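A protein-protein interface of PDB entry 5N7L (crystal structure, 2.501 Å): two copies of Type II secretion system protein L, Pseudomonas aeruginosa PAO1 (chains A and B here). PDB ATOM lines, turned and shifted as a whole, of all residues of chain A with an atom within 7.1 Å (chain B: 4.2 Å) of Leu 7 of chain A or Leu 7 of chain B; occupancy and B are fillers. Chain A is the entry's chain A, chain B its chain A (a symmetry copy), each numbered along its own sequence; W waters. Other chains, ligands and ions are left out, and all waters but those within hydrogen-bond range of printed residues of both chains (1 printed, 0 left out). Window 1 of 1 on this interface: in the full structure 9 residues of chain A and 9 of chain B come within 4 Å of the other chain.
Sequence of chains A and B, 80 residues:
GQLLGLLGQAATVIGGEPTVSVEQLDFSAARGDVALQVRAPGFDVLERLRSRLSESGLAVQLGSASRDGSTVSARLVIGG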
ATOM      1  N   GLN A   2      13.216   7.798 -28.260  1.00  0.00           N
ATOM      2  CA  GLN A   2      12.560   8.408 -29.409  1.00  0.00           C
ATOM      3  C   GLN A   2      11.201   9.005 -29.079  1.00  0.00           C
ATOM      4  O   GLN A   2      10.549   9.546 -29.976  1.00  0.00           O
ATOM      5  CB  GLN A   2      12.390   7.373 -30.533  1.00  0.00           C
ATOM      6  CG  GLN A   2      11.112   6.524 -30.444  1.00  0.00           C
ATOM      7  CD  GLN A   2      10.968   5.779 -29.124  1.00  0.00           C
ATOM      8  OE1 GLN A   2      11.958   5.461 -28.461  1.00  0.00           O
ATOM      9  NE2 GLN A   2       9.729   5.499 -28.736  1.00  0.00           N
ATOM     10  N   LEU A   3      10.760   8.927 -27.826  1.00  0.00           N
ATOM     11  CA  LEU A   3       9.387   9.273 -27.475  1.00  0.00           C
ATOM     12  C   LEU A   3       9.081  10.747 -27.741  1.00  0.00           C
ATOM     13  O   LEU A   3       7.985  11.093 -28.210  1.00  0.00           O
ATOM     14  CB  LEU A   3       9.165   8.907 -26.011  1.00  0.00           C
ATOM     15  CG  LEU A   3       7.920   9.347 -25.258  1.00  0.00           C
ATOM     16  CD1 LEU A   3       7.382   8.224 -24.456  1.00  0.00           C
ATOM     17  CD2 LEU A   3       8.272  10.473 -24.345  1.00  0.00           C
ATOM     18  N   LEU A   4      10.040  11.631 -27.457  1.00  0.00           N
ATOM     19  CA  LEU A   4       9.816  13.050 -27.714  1.00  0.00           C
ATOM     20  C   LEU A   4       9.605  13.319 -29.203  1.00  0.00           C
ATOM     21  O   LEU A   4       8.877  14.249 -29.572  1.00  0.00           O
ATOM     22  CB  LEU A   4      10.987  13.870 -27.166  1.00  0.00           C
ATOM     23  CG  LEU A   4      10.903  15.399 -27.223  1.00  0.00           C
ATOM     24  CD1 LEU A   4      10.063  15.923 -26.073  1.00  0.00           C
ATOM     25  CD2 LEU A   4      12.290  16.025 -27.186  1.00  0.00           C
ATOM     26  N   GLY A   5      10.211  12.508 -30.072  1.00  0.00           N
ATOM     27  CA  GLY A   5       9.896  12.596 -31.489  1.00  0.00           C
ATOM     28  C   GLY A   5       8.461  12.202 -31.784  1.00  0.00           C
ATOM     29  O   GLY A   5       7.804  12.804 -32.640  1.00  0.00           O
ATOM     30  N   LEU A   6       7.955  11.184 -31.081  1.00  0.00           N
ATOM     31  CA  LEU A   6       6.543  10.840 -31.195  1.00  0.00           C
ATOM     32  C   LEU A   6       5.670  12.032 -30.838  1.00  0.00           C
ATOM     33  O   LEU A   6       4.681  12.320 -31.530  1.00  0.00           O
ATOM     34  CB  LEU A   6       6.210   9.645 -30.298  1.00  0.00           C
ATOM     35  CG  LEU A   6       6.978   8.343 -30.524  1.00  0.00           C
ATOM     36  CD1 LEU A   6       6.465   7.256 -29.586  1.00  0.00           C
ATOM     37  CD2 LEU A   6       6.882   7.896 -31.974  1.00  0.00           C
ATOM     38  N   LEU A   7       6.026  12.752 -29.768  1.00  0.00           N
ATOM     39  CA  LEU A   7       5.273  13.965 -29.465  1.00  0.00           C
ATOM     40  C   LEU A   7       5.471  15.017 -30.554  1.00  0.00           C
ATOM     41  O   LEU A   7       4.586  15.847 -30.778  1.00  0.00           O
ATOM     42  CB  LEU A   7       5.666  14.514 -28.090  1.00  0.00           C
ATOM     43  CG  LEU A   7       4.661  15.379 -27.299  1.00  0.00           C
ATOM     44  CD1 LEU A   7       5.163  15.594 -25.876  1.00  0.00           C
ATOM     45  CD2 LEU A   7       4.339  16.732 -27.941  1.00  0.00           C
ATOM     46  N   GLY A   8       6.601  14.985 -31.265  1.00  0.00           N
ATOM     47  CA  GLY A   8       6.768  15.884 -32.399  1.00  0.00           C
ATOM     48  C   GLY A   8       5.766  15.618 -33.507  1.00  0.00           C
ATOM     49  O   GLY A   8       5.063  16.529 -33.963  1.00  0.00           O
ATOM     50  N   GLN A   9       5.691  14.362 -33.961  1.00  0.00           N
ATOM     51  CA  GLN A   9       4.729  14.004 -35.000  1.00  0.00           C
ATOM     52  C   GLN A   9       3.305  14.314 -34.556  1.00  0.00           C
ATOM     53  O   GLN A   9       2.526  14.932 -35.298  1.00  0.00           O
ATOM     54  CB  GLN A   9       4.871  12.524 -35.357  1.00  0.00           C
ATOM     55  CG  GLN A   9       6.307  12.052 -35.512  1.00  0.00           C
ATOM     56  CD  GLN A   9       6.394  10.643 -36.061  1.00  0.00           C
ATOM     57  OE1 GLN A   9       5.488  10.183 -36.756  1.00  0.00           O
ATOM     58  NE2 GLN A   9       7.483   9.950 -35.750  1.00  0.00           N
ATOM     59  N   ALA A  10       2.948  13.892 -33.339  1.00  0.00           N
ATOM     60  CA  ALA A  10       1.635  14.229 -32.802  1.00  0.00           C
ATOM     61  C   ALA A  10       1.410  15.734 -32.789  1.00  0.00           C
ATOM     62  O   ALA A  10       0.283  16.194 -32.992  1.00  0.00           O
ATOM     63  CB  ALA A  10       1.477  13.654 -31.396  1.00  0.00           C
ATOM     64  N   ALA A  11       2.468  16.516 -32.569  1.00  0.00           N
ATOM     65  CA  ALA A  11       2.327  17.965 -32.556  1.00  0.00           C
ATOM     66  C   ALA A  11       2.011  18.496 -33.946  1.00  0.00           C
ATOM     67  O   ALA A  11       1.219  19.433 -34.091  1.00  0.00           O
ATOM     68  CB  ALA A  11       3.596  18.612 -32.004  1.00  0.00           C
ATOM     69  N   THR A  12       2.620  17.915 -34.983  1.00  0.00           N
ATOM     70  CA  THR A  12       2.267  18.306 -36.345  1.00  0.00           C
ATOM     71  C   THR A  12       0.811  17.960 -36.651  1.00  0.00           C
ATOM     72  O   THR A  12       0.032  18.818 -37.093  1.00  0.00           O
ATOM     73  CB  THR A  12       3.202  17.631 -37.349  1.00  0.00           C
ATOM     74  OG1 THR A  12       4.560  17.971 -37.047  1.00  0.00           O
ATOM     75  CG2 THR A  12       2.874  18.083 -38.766  1.00  0.00           C
ATOM     76  N   VAL A  13       0.425  16.705 -36.401  1.00  0.00           N
ATOM     77  CA  VAL A  13      -0.922  16.252 -36.741  1.00  0.00           C
ATOM     78  C   VAL A  13      -1.972  17.076 -36.002  1.00  0.00           C
ATOM     79  O   VAL A  13      -2.925  17.585 -36.603  1.00  0.00           O
ATOM     80  CB  VAL A  13      -1.073  14.750 -36.443  1.00  0.00           C
ATOM     81  CG1 VAL A  13      -2.496  14.292 -36.725  1.00  0.00           C
ATOM     82  CG2 VAL A  13      -0.074  13.945 -37.260  1.00  0.00           C
ATOM     83  N   ILE A  14      -1.811  17.220 -34.684  1.00  0.00           N
ATOM     84  CA  ILE A  14      -2.769  17.990 -33.897  1.00  0.00           C
ATOM     85  C   ILE A  14      -2.741  19.458 -34.300  1.00  0.00           C
ATOM     86  O   ILE A  14      -3.779  20.131 -34.296  1.00  0.00           O
ATOM     87  CB  ILE A  14      -2.490  17.802 -32.393  1.00  0.00           C
ATOM     88  CG1 ILE A  14      -2.649  16.330 -32.008  1.00  0.00           C
ATOM     89  CG2 ILE A  14      -3.416  18.671 -31.554  1.00  0.00           C
ATOM     90  CD1 ILE A  14      -2.201  16.015 -30.601  1.00  0.00           C
ATOM     91  N   LEU A  25      -1.012  17.460 -20.795  1.00  0.00           N
ATOM     92  CA  LEU A  25      -0.286  16.281 -21.240  1.00  0.00           C
ATOM     93  C   LEU A  25       0.581  15.759 -20.107  1.00  0.00           C
ATOM     94  O   LEU A  25       0.981  16.502 -19.206  1.00  0.00           O
ATOM     95  CB  LEU A  25       0.542  16.543 -22.511  1.00  0.00           C
ATOM     96  CG  LEU A  25       1.904  17.227 -22.610  1.00  0.00           C
ATOM     97  CD1 LEU A  25       3.045  16.329 -22.165  1.00  0.00           C
ATOM     98  CD2 LEU A  25       2.104  17.608 -24.061  1.00  0.00           C
ATOM     99  N   PHE A  27       3.754  13.301 -19.811  1.00  0.00           N
ATOM    100  CA  PHE A  27       4.895  12.734 -20.516  1.00  0.00           C
ATOM    101  C   PHE A  27       5.604  11.774 -19.568  1.00  0.00           C
ATOM    102  O   PHE A  27       6.116  12.197 -18.525  1.00  0.00           O
ATOM    103  CB  PHE A  27       5.780  13.902 -20.962  1.00  0.00           C
ATOM    104  CG  PHE A  27       7.155  13.539 -21.479  1.00  0.00           C
ATOM    105  CD1 PHE A  27       7.450  13.672 -22.818  1.00  0.00           C
ATOM    106  CD2 PHE A  27       8.171  13.156 -20.619  1.00  0.00           C
ATOM    107  CE1 PHE A  27       8.721  13.422 -23.284  1.00  0.00           C
ATOM    108  CE2 PHE A  27       9.440  12.865 -21.086  1.00  0.00           C
ATOM    109  CZ  PHE A  27       9.712  12.994 -22.414  1.00  0.00           C
ATOM    110  N   VAL A  34       3.008   9.117 -23.804  1.00  0.00           N
ATOM    111  CA  VAL A  34       2.591  10.470 -23.455  1.00  0.00           C
ATOM    112  C   VAL A  34       1.074  10.541 -23.577  1.00  0.00           C
ATOM    113  O   VAL A  34       0.490  10.012 -24.529  1.00  0.00           O
ATOM    114  CB  VAL A  34       3.287  11.530 -24.340  1.00  0.00           C
ATOM    115  CG1 VAL A  34       2.991  11.290 -25.815  1.00  0.00           C
ATOM    116  CG2 VAL A  34       2.867  12.933 -23.925  1.00  0.00           C
ATOM    117  N   LEU A  36      -2.389  12.942 -23.709  1.00  0.00           N
ATOM    118  CA  LEU A  36      -2.862  14.274 -24.064  1.00  0.00           C
ATOM    119  C   LEU A  36      -4.330  14.387 -23.682  1.00  0.00           C
ATOM    120  O   LEU A  36      -5.157  13.595 -24.145  1.00  0.00           O
ATOM    121  CB  LEU A  36      -2.679  14.544 -25.560  1.00  0.00           C
ATOM    122  CG  LEU A  36      -1.263  14.497 -26.139  1.00  0.00           C
ATOM    123  CD1 LEU A  36      -1.026  13.177 -26.832  1.00  0.00           C
ATOM    124  CD2 LEU A  36      -1.054  15.646 -27.118  1.00  0.00           C
ATOM    125  N   LEU A  58       1.831   6.437 -35.933  1.00  0.00           N
ATOM    126  CA  LEU A  58       1.864   6.425 -34.478  1.00  0.00           C
ATOM    127  C   LEU A  58       0.868   5.422 -33.911  1.00  0.00           C
ATOM    128  O   LEU A  58      -0.229   5.235 -34.448  1.00  0.00           O
ATOM    129  CB  LEU A  58       1.555   7.816 -33.924  1.00  0.00           C
ATOM    130  CG  LEU A  58       2.396   8.987 -34.433  1.00  0.00           C
ATOM    131  CD1 LEU A  58       1.892  10.296 -33.847  1.00  0.00           C
ATOM    132  CD2 LEU A  58       3.863   8.778 -34.099  1.00  0.00           C
ATOM    133  N   ILE A  78      -0.350   8.381 -26.767  1.00  0.00           N
ATOM    134  CA  ILE A  78       0.589   8.091 -27.844  1.00  0.00           C
ATOM    135  C   ILE A  78       1.742   7.284 -27.265  1.00  0.00           C
ATOM    136  O   ILE A  78       2.320   7.665 -26.239  1.00  0.00           O
ATOM    137  CB  ILE A  78       1.110   9.381 -28.501  1.00  0.00           C
ATOM    138  CG1 ILE A  78      -0.031  10.366 -28.748  1.00  0.00           C
ATOM    139  CG2 ILE A  78       1.834   9.064 -29.800  1.00  0.00           C
ATOM    140  CD1 ILE A  78      -0.980   9.941 -29.835  1.00  0.00           C
ATOM    141  N   LEU B   3       1.351  26.555 -28.491  1.00  0.00           N
ATOM    142  CA  LEU B   3       2.424  26.095 -27.616  1.00  0.00           C
ATOM    143  C   LEU B   3       2.879  24.678 -27.964  1.00  0.00           C
ATOM    144  O   LEU B   3       4.082  24.373 -27.931  1.00  0.00           O
ATOM    145  CB  LEU B   3       1.934  26.191 -26.174  1.00  0.00           C
ATOM    146  CG  LEU B   3       2.714  25.575 -25.024  1.00  0.00           C
ATOM    147  CD1 LEU B   3       2.775  26.516 -23.883  1.00  0.00           C
ATOM    148  CD2 LEU B   3       2.031  24.323 -24.586  1.00  0.00           C
ATOM    149  N   LEU B   4       1.936  23.800 -28.310  1.00  0.00           N
ATOM    150  CA  LEU B   4       2.313  22.439 -28.678  1.00  0.00           C
ATOM    151  C   LEU B   4       3.194  22.425 -29.926  1.00  0.00           C
ATOM    152  O   LEU B   4       4.050  21.543 -30.076  1.00  0.00           O
ATOM    153  CB  LEU B   4       1.058  21.587 -28.879  1.00  0.00           C
ATOM    154  CG  LEU B   4       1.223  20.089 -29.157  1.00  0.00           C
ATOM    155  CD1 LEU B   4       1.464  19.337 -27.861  1.00  0.00           C
ATOM    156  CD2 LEU B   4       0.002  19.526 -29.869  1.00  0.00           C
ATOM    157  N   GLY B   5       3.019  23.400 -30.820  1.00  0.00           N
ATOM    158  CA  GLY B   5       3.953  23.546 -31.926  1.00  0.00           C
ATOM    159  C   GLY B   5       5.345  23.924 -31.457  1.00  0.00           C
ATOM    160  O   GLY B   5       6.346  23.452 -32.007  1.00  0.00           O
ATOM    161  N   LEU B   6       5.428  24.781 -30.436  1.00  0.00           N
ATOM    162  CA  LEU B   6       6.720  25.079 -29.828  1.00  0.00           C
ATOM    163  C   LEU B   6       7.382  23.808 -29.324  1.00  0.00           C
ATOM    164  O   LEU B   6       8.590  23.603 -29.524  1.00  0.00           O
ATOM    165  CB  LEU B   6       6.553  26.085 -28.686  1.00  0.00           C
ATOM    166  CG  LEU B   6       5.920  27.439 -29.008  1.00  0.00           C
ATOM    167  CD1 LEU B   6       5.900  28.322 -27.767  1.00  0.00           C
ATOM    168  CD2 LEU B   6       6.651  28.126 -30.150  1.00  0.00           C
ATOM    169  N   LEU B   7       6.607  22.929 -28.680  1.00  0.00           N
ATOM    170  CA  LEU B   7       7.188  21.651 -28.281  1.00  0.00           C
ATOM    171  C   LEU B   7       7.556  20.813 -29.504  1.00  0.00           C
ATOM    172  O   LEU B   7       8.479  19.998 -29.439  1.00  0.00           O
ATOM    173  CB  LEU B   7       6.232  20.888 -27.359  1.00  0.00           C
ATOM    174  CG  LEU B   7       6.800  19.856 -26.359  1.00  0.00           C
ATOM    175  CD1 LEU B   7       5.710  19.419 -25.386  1.00  0.00           C
ATOM    176  CD2 LEU B   7       7.437  18.623 -27.007  1.00  0.00           C
ATOM    177  N   GLY B   8       6.877  21.016 -30.637  1.00  0.00           N
ATOM    178  CA  GLY B   8       7.287  20.336 -31.859  1.00  0.00           C
ATOM    179  C   GLY B   8       8.672  20.748 -32.318  1.00  0.00           C
ATOM    180  O   GLY B   8       9.545  19.902 -32.553  1.00  0.00           O
ATOM    181  N   GLN B   9       8.894  22.059 -32.462  1.00  0.00           N
ATOM    182  CA  GLN B   9      10.208  22.551 -32.864  1.00  0.00           C
ATOM    183  C   GLN B   9      11.283  22.109 -31.879  1.00  0.00           C
ATOM    184  O   GLN B   9      12.341  21.596 -32.276  1.00  0.00           O
ATOM    185  CB  GLN B   9      10.184  24.075 -32.983  1.00  0.00           C
ATOM    186  CG  GLN B   9       8.959  24.628 -33.694  1.00  0.00           C
ATOM    187  CD  GLN B   9       9.074  26.114 -33.967  1.00  0.00           C
ATOM    188  OE1 GLN B   9      10.177  26.649 -34.078  1.00  0.00           O
ATOM    189  NE2 GLN B   9       7.935  26.788 -34.074  1.00  0.00           N
ATOM    190  N   ALA B  10      11.024  22.297 -30.581  1.00  0.00           N
ATOM    191  CA  ALA B  10      11.958  21.816 -29.570  1.00  0.00           C
ATOM    192  C   ALA B  10      12.216  20.323 -29.717  1.00  0.00           C
ATOM    193  O   ALA B  10      13.330  19.858 -29.457  1.00  0.00           O
ATOM    194  CB  ALA B  10      11.430  22.130 -28.171  1.00  0.00           C
ATOM    195  N   ALA B  11      11.209  19.561 -30.146  1.00  0.00           N
ATOM    196  CA  ALA B  11      11.390  18.127 -30.322  1.00  0.00           C
ATOM    197  C   ALA B  11      12.330  17.833 -31.481  1.00  0.00           C
ATOM    198  O   ALA B  11      13.140  16.903 -31.407  1.00  0.00           O
ATOM    199  CB  ALA B  11      10.038  17.448 -30.535  1.00  0.00           C
ATOM    200  N   LEU B  25       8.944  16.436 -18.453  1.00  0.00           N
ATOM    201  CA  LEU B  25       8.453  17.704 -18.969  1.00  0.00           C
ATOM    202  C   LEU B  25       7.142  18.057 -18.287  1.00  0.00           C
ATOM    203  O   LEU B  25       6.406  17.187 -17.814  1.00  0.00           O
ATOM    204  CB  LEU B  25       8.312  17.703 -20.501  1.00  0.00           C
ATOM    205  CG  LEU B  25       7.177  17.105 -21.330  1.00  0.00           C
ATOM    206  CD1 LEU B  25       5.922  17.960 -21.309  1.00  0.00           C
ATOM    207  CD2 LEU B  25       7.680  16.991 -22.753  1.00  0.00           C
ATOM    208  N   VAL B  34       6.399  25.338 -21.466  1.00  0.00           N
ATOM    209  CA  VAL B  34       6.666  23.928 -21.206  1.00  0.00           C
ATOM    210  C   VAL B  34       8.072  23.815 -20.630  1.00  0.00           C
ATOM    211  O   VAL B  34       9.004  24.477 -21.100  1.00  0.00           O
ATOM    212  CB  VAL B  34       6.499  23.070 -22.481  1.00  0.00           C
ATOM    213  CG1 VAL B  34       7.428  23.550 -23.590  1.00  0.00           C
ATOM    214  CG2 VAL B  34       6.741  21.599 -22.171  1.00  0.00           C
HETATM  215  O   HOH W   1       7.119  14.365 -17.085  1.00  0.00           O
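Water W1 lies within hydrogen-bond range of O of Phe 27 of chain A (2.8 Å) and O of Leu 25 of chain B (3.0 Å).
Leu 4 of chain A touches Leu 7 of chain B.
Ala 11 of chain B touches Leu 4 of chain A (CB to O, 3.5 Å).
CD2 of Leu 7 of chain A touches CD1 of Leu 4 of chain B, at 3.9 Å.
Leu 7 of chain A touches Leu 7 of chain B (CD2 to CD2, 3.7 Å).
CB of Ala 11 of chain A touches O of Leu 4 of chain B, at 3.5 Å.
Leu 4 of chain B touches Ile 14 of chain A.
CD1 of Leu 25 of chain B touches CD1 of Leu 25 of chain A, at 3.4 Å.
Phe 27 of chain A touches Leu 25 of chain B (CD1 to CD2, 3.3 Å).
Of the 19 printed residues of chain A, 6 touch a printed residue of chain B.
Hydrophobic or aromatic side chains of chain A that line the printed part of chain B: Leu 4, Leu 7, Ala 11, Ile 14, Leu 25 and Phe 27.
Hydrophobic or aromatic side chains of chain B that line the printed part of chain A: Leu 4, Leu 7, Ala 11 and Leu 25.
Along chain B the printed residues that touch a printed residue of chain A span positions 4 to 25.
Among the printed residues, 8 pairs touch across the chains.
Among the printed residues, no Asp or Glu carboxylate lies within 4 Å of a Lys or Arg side-chain nitrogen of the other chain.
Leu 4 of chain A touches Leu 7 of chain B, and with the chains exchanged Leu 7 of chain A touches Leu 4 of chain B.
Leu 4 of chain A touches Ala 11 of chain B, and with the chains exchanged Ala 11 of chain A touches Leu 4 of chain B.
Leu 7 of chain B touches its own counterpart, Leu 7 of chain A.
Leu 25 of chain A touches its own counterpart, Leu 25 of chain B.
Of the 8 pairs that touch across the chains among the printed residues, 6 have their exchanged pair printed and touching as well.
Of the printed residues of chain B, Leu 7 of chain A touches Leu 4 (3.9 Å) and Leu 7 (3.7 Å).
Of the printed residues of chain A, Leu 7 of chain B touches Leu 4 (3.9 Å) and Leu 7 (3.7 Å).
Of the printed residues of chain A, Leu 4 of chain B touches Leu 7 (3.9 Å), Ala 11 (3.5 Å) and Ile 14 (3.9 Å).
Printed residues of chain B within 4 Å of Leu 25 of chain A: Leu 25 (3.4 Å).
The nearest printed residue of chain B that does not touch Leu 7 of chain A is Leu 25 of chain B (4.2 Å).
The nearest printed residue of chain A that does not touch Leu 7 of chain B is Leu 25 of chain A (4.2 Å).
The nearest printed residue of chain B that does not touch Leu 4 of chain A is Leu 25 of chain B (4.2 Å).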
